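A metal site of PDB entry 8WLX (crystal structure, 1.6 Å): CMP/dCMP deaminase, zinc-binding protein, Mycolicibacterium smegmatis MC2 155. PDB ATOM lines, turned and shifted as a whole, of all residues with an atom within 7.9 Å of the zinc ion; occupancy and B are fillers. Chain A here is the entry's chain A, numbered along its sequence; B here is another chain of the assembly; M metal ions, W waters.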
ATOM      1  N   PHE A  28      12.962 -16.119 -13.602  1.00  0.00           N
ATOM      2  CA  PHE A  28      12.026 -17.229 -13.562  1.00  0.00           C
ATOM      3  C   PHE A  28      10.639 -16.702 -13.889  1.00  0.00           C
ATOM      4  O   PHE A  28      10.173 -15.712 -13.310  1.00  0.00           O
ATOM      5  CB  PHE A  28      12.040 -17.884 -12.175  1.00  0.00           C
ATOM      6  CG  PHE A  28      13.376 -18.441 -11.752  1.00  0.00           C
ATOM      7  CD1 PHE A  28      13.733 -19.734 -12.049  1.00  0.00           C
ATOM      8  CD2 PHE A  28      14.242 -17.677 -11.004  1.00  0.00           C
ATOM      9  CE1 PHE A  28      14.968 -20.212 -11.654  1.00  0.00           C
ATOM     10  CE2 PHE A  28      15.453 -18.165 -10.556  1.00  0.00           C
ATOM     11  CZ  PHE A  28      15.815 -19.446 -10.893  1.00  0.00           C
ATOM     12  N   ASN A  45       9.278 -14.207 -10.940  1.00  0.00           N
ATOM     13  CA  ASN A  45       9.947 -14.078  -9.654  1.00  0.00           C
ATOM     14  C   ASN A  45       9.833 -12.631  -9.136  1.00  0.00           C
ATOM     15  O   ASN A  45      10.050 -11.672  -9.896  1.00  0.00           O
ATOM     16  CB  ASN A  45      11.376 -14.529  -9.804  1.00  0.00           C
ATOM     17  CG  ASN A  45      12.168 -14.362  -8.541  1.00  0.00           C
ATOM     18  OD1 ASN A  45      12.627 -13.247  -8.232  1.00  0.00           O
ATOM     19  ND2 ASN A  45      12.465 -15.476  -7.902  1.00  0.00           N
ATOM     20  N   ALA A  52      12.483 -14.620  -0.326  1.00  0.00           N
ATOM     21  CA  ALA A  52      13.087 -15.608  -1.205  1.00  0.00           C
ATOM     22  C   ALA A  52      12.048 -16.646  -1.664  1.00  0.00           C
ATOM     23  O   ALA A  52      12.365 -17.377  -2.590  1.00  0.00           O
ATOM     24  CB  ALA A  52      14.218 -16.308  -0.496  1.00  0.00           C
ATOM     25  N   THR A  53      10.851 -16.712  -1.051  1.00  0.00           N
ATOM     26  CA  THR A  53       9.832 -17.683  -1.488  1.00  0.00           C
ATOM     27  C   THR A  53       8.924 -17.086  -2.566  1.00  0.00           C
ATOM     28  O   THR A  53       7.963 -17.749  -2.972  1.00  0.00           O
ATOM     29  CB  THR A  53       8.987 -18.179  -0.326  1.00  0.00           C
ATOM     30  OG1 THR A  53       8.142 -17.107   0.111  1.00  0.00           O
ATOM     31  CG2 THR A  53       9.796 -18.751   0.820  1.00  0.00           C
ATOM     32  N   ALA A  54       9.205 -15.862  -3.069  1.00  0.00           N
ATOM     33  CA  ALA A  54       8.342 -15.265  -4.081  1.00  0.00           C
ATOM     34  C   ALA A  54       8.569 -15.839  -5.480  1.00  0.00           C
ATOM     35  O   ALA A  54       8.911 -15.140  -6.469  1.00  0.00           O
ATOM     36  CB  ALA A  54       8.576 -13.739  -4.093  1.00  0.00           C
ATOM     37  N   HIS A  55       8.285 -17.139  -5.618  1.00  0.00           N
ATOM     38  CA  HIS A  55       8.408 -17.829  -6.872  1.00  0.00           C
ATOM     39  C   HIS A  55       7.090 -17.831  -7.619  1.00  0.00           C
ATOM     40  O   HIS A  55       6.026 -18.038  -7.036  1.00  0.00           O
ATOM     41  CB  HIS A  55       8.778 -19.291  -6.584  1.00  0.00           C
ATOM     42  CG  HIS A  55      10.088 -19.467  -5.927  1.00  0.00           C
ATOM     43  ND1 HIS A  55      10.713 -20.714  -5.874  1.00  0.00           N
ATOM     44  CD2 HIS A  55      10.945 -18.582  -5.331  1.00  0.00           C
ATOM     45  CE1 HIS A  55      11.888 -20.567  -5.225  1.00  0.00           C
ATOM     46  NE2 HIS A  55      12.058 -19.268  -4.888  1.00  0.00           N
ATOM     47  N   PRO A  56       7.144 -17.763  -8.952  1.00  0.00           N
ATOM     48  CA  PRO A  56       5.890 -17.655  -9.695  1.00  0.00           C
ATOM     49  C   PRO A  56       5.052 -18.922  -9.671  1.00  0.00           C
ATOM     50  O   PRO A  56       3.842 -18.863  -9.693  1.00  0.00           O
ATOM     51  CB  PRO A  56       6.366 -17.272 -11.076  1.00  0.00           C
ATOM     52  CG  PRO A  56       7.754 -17.792 -11.185  1.00  0.00           C
ATOM     53  CD  PRO A  56       8.347 -17.598  -9.787  1.00  0.00           C
ATOM     54  N   GLU A  57       5.698 -20.109  -9.658  1.00  0.00           N
ATOM     55  CA  GLU A  57       4.931 -21.339  -9.635  1.00  0.00           C
ATOM     56  C   GLU A  57       4.103 -21.433  -8.354  1.00  0.00           C
ATOM     57  O   GLU A  57       3.031 -22.032  -8.333  1.00  0.00           O
ATOM     58  CB  GLU A  57       5.864 -22.543  -9.757  1.00  0.00           C
ATOM     59  CG  GLU A  57       6.874 -22.546 -10.907  1.00  0.00           C
ATOM     60  CD  GLU A  57       8.228 -22.056 -10.369  1.00  0.00           C
ATOM     61  OE1 GLU A  57       8.348 -20.899  -9.925  1.00  0.00           O
ATOM     62  OE2 GLU A  57       9.143 -22.900 -10.202  1.00  0.00           O
ATOM     63  N   PHE A  58       4.665 -20.956  -7.227  1.00  0.00           N
ATOM     64  CA  PHE A  58       3.941 -20.931  -5.970  1.00  0.00           C
ATOM     65  C   PHE A  58       2.745 -19.999  -6.018  1.00  0.00           C
ATOM     66  O   PHE A  58       1.638 -20.349  -5.587  1.00  0.00           O
ATOM     67  CB  PHE A  58       4.916 -20.547  -4.834  1.00  0.00           C
ATOM     68  CG  PHE A  58       4.253 -20.740  -3.483  1.00  0.00           C
ATOM     69  CD1 PHE A  58       4.211 -21.998  -2.890  1.00  0.00           C
ATOM     70  CD2 PHE A  58       3.511 -19.720  -2.898  1.00  0.00           C
ATOM     71  CE1 PHE A  58       3.522 -22.183  -1.704  1.00  0.00           C
ATOM     72  CE2 PHE A  58       2.850 -19.910  -1.695  1.00  0.00           C
ATOM     73  CZ  PHE A  58       2.812 -21.160  -1.128  1.00  0.00           C
ATOM     74  N   GLY A  82      12.041 -22.447 -15.588  1.00  0.00           N
ATOM     75  CA  GLY A  82      12.916 -23.294 -14.788  1.00  0.00           C
ATOM     76  C   GLY A  82      12.111 -24.283 -13.965  1.00  0.00           C
ATOM     77  O   GLY A  82      11.108 -23.924 -13.379  1.00  0.00           O
ATOM     78  N   GLU A  83      12.509 -25.556 -14.012  1.00  0.00           N
ATOM     79  CA  GLU A  83      11.804 -26.606 -13.281  1.00  0.00           C
ATOM     80  C   GLU A  83      11.540 -26.164 -11.844  1.00  0.00           C
ATOM     81  O   GLU A  83      12.435 -25.667 -11.163  1.00  0.00           O
ATOM     82  CB  GLU A  83      12.698 -27.859 -13.303  1.00  0.00           C
ATOM     83  CG  GLU A  83      12.156 -29.040 -12.514  1.00  0.00           C
ATOM     84  CD  GLU A  83      12.972 -30.313 -12.567  1.00  0.00           C
ATOM     85  OE1 GLU A  83      14.183 -30.238 -12.922  1.00  0.00           O
ATOM     86  OE2 GLU A  83      12.384 -31.393 -12.171  1.00  0.00           O
ATOM     87  N   HIS A  84      10.321 -26.458 -11.361  1.00  0.00           N
ATOM     88  CA  HIS A  84       9.880 -26.154 -10.020  1.00  0.00           C
ATOM     89  C   HIS A  84      10.937 -26.616  -9.007  1.00  0.00           C
ATOM     90  O   HIS A  84      11.311 -27.806  -9.025  1.00  0.00           O
ATOM     91  CB  HIS A  84       8.591 -26.918  -9.728  1.00  0.00           C
ATOM     92  CG  HIS A  84       7.382 -26.454 -10.480  1.00  0.00           C
ATOM     93  ND1 HIS A  84       7.422 -26.284 -11.852  1.00  0.00           N
ATOM     94  CD2 HIS A  84       6.147 -26.154 -10.086  1.00  0.00           C
ATOM     95  CE1 HIS A  84       6.210 -25.906 -12.250  1.00  0.00           C
ATOM     96  NE2 HIS A  84       5.407 -25.781 -11.206  1.00  0.00           N
ATOM     97  N   CYS A  85      11.257 -25.759  -8.057  1.00  0.00           N
ATOM     98  CA  CYS A  85      11.961 -26.154  -6.852  1.00  0.00           C
ATOM     99  C   CYS A  85      11.025 -26.993  -5.989  1.00  0.00           C
ATOM    100  O   CYS A  85       9.827 -27.009  -6.224  1.00  0.00           O
ATOM    101  CB  CYS A  85      12.464 -24.951  -6.027  1.00  0.00           C
ATOM    102  SG  CYS A  85      11.220 -24.092  -5.025  1.00  0.00           S
ATOM    103  N   PRO A  86      11.542 -27.681  -4.933  1.00  0.00           N
ATOM    104  CA  PRO A  86      10.685 -28.525  -4.113  1.00  0.00           C
ATOM    105  C   PRO A  86       9.517 -27.799  -3.488  1.00  0.00           C
ATOM    106  O   PRO A  86       8.469 -28.388  -3.290  1.00  0.00           O
ATOM    107  CB  PRO A  86      11.642 -29.112  -3.091  1.00  0.00           C
ATOM    108  CG  PRO A  86      12.944 -29.222  -3.859  1.00  0.00           C
ATOM    109  CD  PRO A  86      12.957 -27.934  -4.663  1.00  0.00           C
ATOM    110  N   MET A  87       9.711 -26.532  -3.120  1.00  0.00           N
ATOM    111  CA  MET A  87       8.636 -25.749  -2.548  1.00  0.00           C
ATOM    112  C   MET A  87       7.441 -25.700  -3.500  1.00  0.00           C
ATOM    113  O   MET A  87       6.282 -25.921  -3.143  1.00  0.00           O
ATOM    114  CB  MET A  87       9.087 -24.299  -2.283  1.00  0.00           C
ATOM    115  CG  MET A  87       8.133 -23.490  -1.455  1.00  0.00           C
ATOM    116  SD  MET A  87       8.656 -21.787  -1.181  1.00  0.00           S
ATOM    117  CE  MET A  87       8.482 -21.213  -2.882  1.00  0.00           C
ATOM    118  N   CYS A  88       7.767 -25.350  -4.742  1.00  0.00           N
ATOM    119  CA  CYS A  88       6.770 -25.130  -5.794  1.00  0.00           C
ATOM    120  C   CYS A  88       6.185 -26.449  -6.307  1.00  0.00           C
ATOM    121  O   CYS A  88       4.981 -26.480  -6.623  1.00  0.00           O
ATOM    122  CB  CYS A  88       7.428 -24.332  -6.902  1.00  0.00           C
ATOM    123  SG  CYS A  88       7.793 -22.633  -6.399  1.00  0.00           S
ATOM    124  N   ALA A  89       7.004 -27.496  -6.436  1.00  0.00           N
ATOM    125  CA  ALA A  89       6.521 -28.790  -6.898  1.00  0.00           C
ATOM    126  C   ALA A  89       5.502 -29.325  -5.884  1.00  0.00           C
ATOM    127  O   ALA A  89       4.441 -29.852  -6.234  1.00  0.00           O
ATOM    128  CB  ALA A  89       7.682 -29.732  -7.044  1.00  0.00           C
ATOM    129  N   VAL A 123      18.304 -25.143  -0.727  1.00  0.00           N
ATOM    130  CA  VAL A 123      17.281 -26.128  -1.064  1.00  0.00           C
ATOM    131  C   VAL A 123      17.807 -27.036  -2.168  1.00  0.00           C
ATOM    132  O   VAL A 123      18.376 -26.580  -3.166  1.00  0.00           O
ATOM    133  CB  VAL A 123      15.966 -25.465  -1.490  1.00  0.00           C
ATOM    134  CG1 VAL A 123      14.954 -26.488  -2.015  1.00  0.00           C
ATOM    135  CG2 VAL A 123      15.364 -24.630  -0.381  1.00  0.00           C
ATOM    136  N   ALA B  90      11.347 -26.501   2.290  1.00  0.00           N
ATOM    137  CA  ALA B  90      12.004 -25.686   1.291  1.00  0.00           C
ATOM    138  C   ALA B  90      11.811 -24.211   1.620  1.00  0.00           C
ATOM    139  O   ALA B  90      12.782 -23.451   1.594  1.00  0.00           O
ATOM    140  CB  ALA B  90      11.463 -26.020  -0.081  1.00  0.00           C
ATOM    141  N   TRP B  94      14.723 -21.527   2.255  1.00  0.00           N
ATOM    142  CA  TRP B  94      14.830 -20.362   1.375  1.00  0.00           C
ATOM    143  C   TRP B  94      14.934 -19.057   2.180  1.00  0.00           C
ATOM    144  O   TRP B  94      15.695 -18.158   1.800  1.00  0.00           O
ATOM    145  CB  TRP B  94      13.676 -20.250   0.358  1.00  0.00           C
ATOM    146  CG  TRP B  94      13.679 -21.196  -0.825  1.00  0.00           C
ATOM    147  CD1 TRP B  94      12.617 -21.937  -1.282  1.00  0.00           C
ATOM    148  CD2 TRP B  94      14.743 -21.436  -1.768  1.00  0.00           C
ATOM    149  NE1 TRP B  94      12.928 -22.592  -2.447  1.00  0.00           N
ATOM    150  CE2 TRP B  94      14.241 -22.318  -2.752  1.00  0.00           C
ATOM    151  CE3 TRP B  94      16.068 -20.990  -1.865  1.00  0.00           C
ATOM    152  CZ2 TRP B  94      15.012 -22.742  -3.821  1.00  0.00           C
ATOM    153  CZ3 TRP B  94      16.826 -21.418  -2.937  1.00  0.00           C
ATOM    154  CH2 TRP B  94      16.300 -22.294  -3.892  1.00  0.00           C
HETATM  155 ZN    ZN M   1      10.072 -22.581  -6.370  1.00  0.00          ZN
HETATM  156  O   HOH W   1      10.735 -22.886  -8.141  1.00  0.00           O
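The backbone carbonyl oxygen of Ala 52 sits at hydrogen-bond distance from a ring nitrogen (NE2) of His 55 (3.0 Å).
The backbone NH of Phe 58 sits close to the side-chain sulfur of Cys 88.
The backbone NH of Met 87 sits close to the side-chain sulfur of Cys 85, 3.4 Å away.
The side-chain sulfur of Cys 85 lies close to the indole nitrogen of Trp 94 of chain B (3.4 Å).
Glu 57 touches the zinc ion.
Four residues have an atom within 4 Å of the zinc ion: His 55, Glu 57, Cys 85 and Cys 88.
Along chain A the residues within 4 Å of the zinc ion span positions 55 to 88.
The nearest printed residue that does not touch the zinc ion is Met 87 (4.1 Å).
The zinc ion is bound by water W1 (1.9 Å), ND1 of His 55 (2.0 Å), SG of Cys 88 (2.3 Å) and SG of Cys 85 (2.3 Å).
The zinc ion has four donor atoms within binding distance.
Water W1 bridges the side-chain carboxylate of Glu 57 (2.6 Å) and the backbone NH of Cys 85 (2.9 Å).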
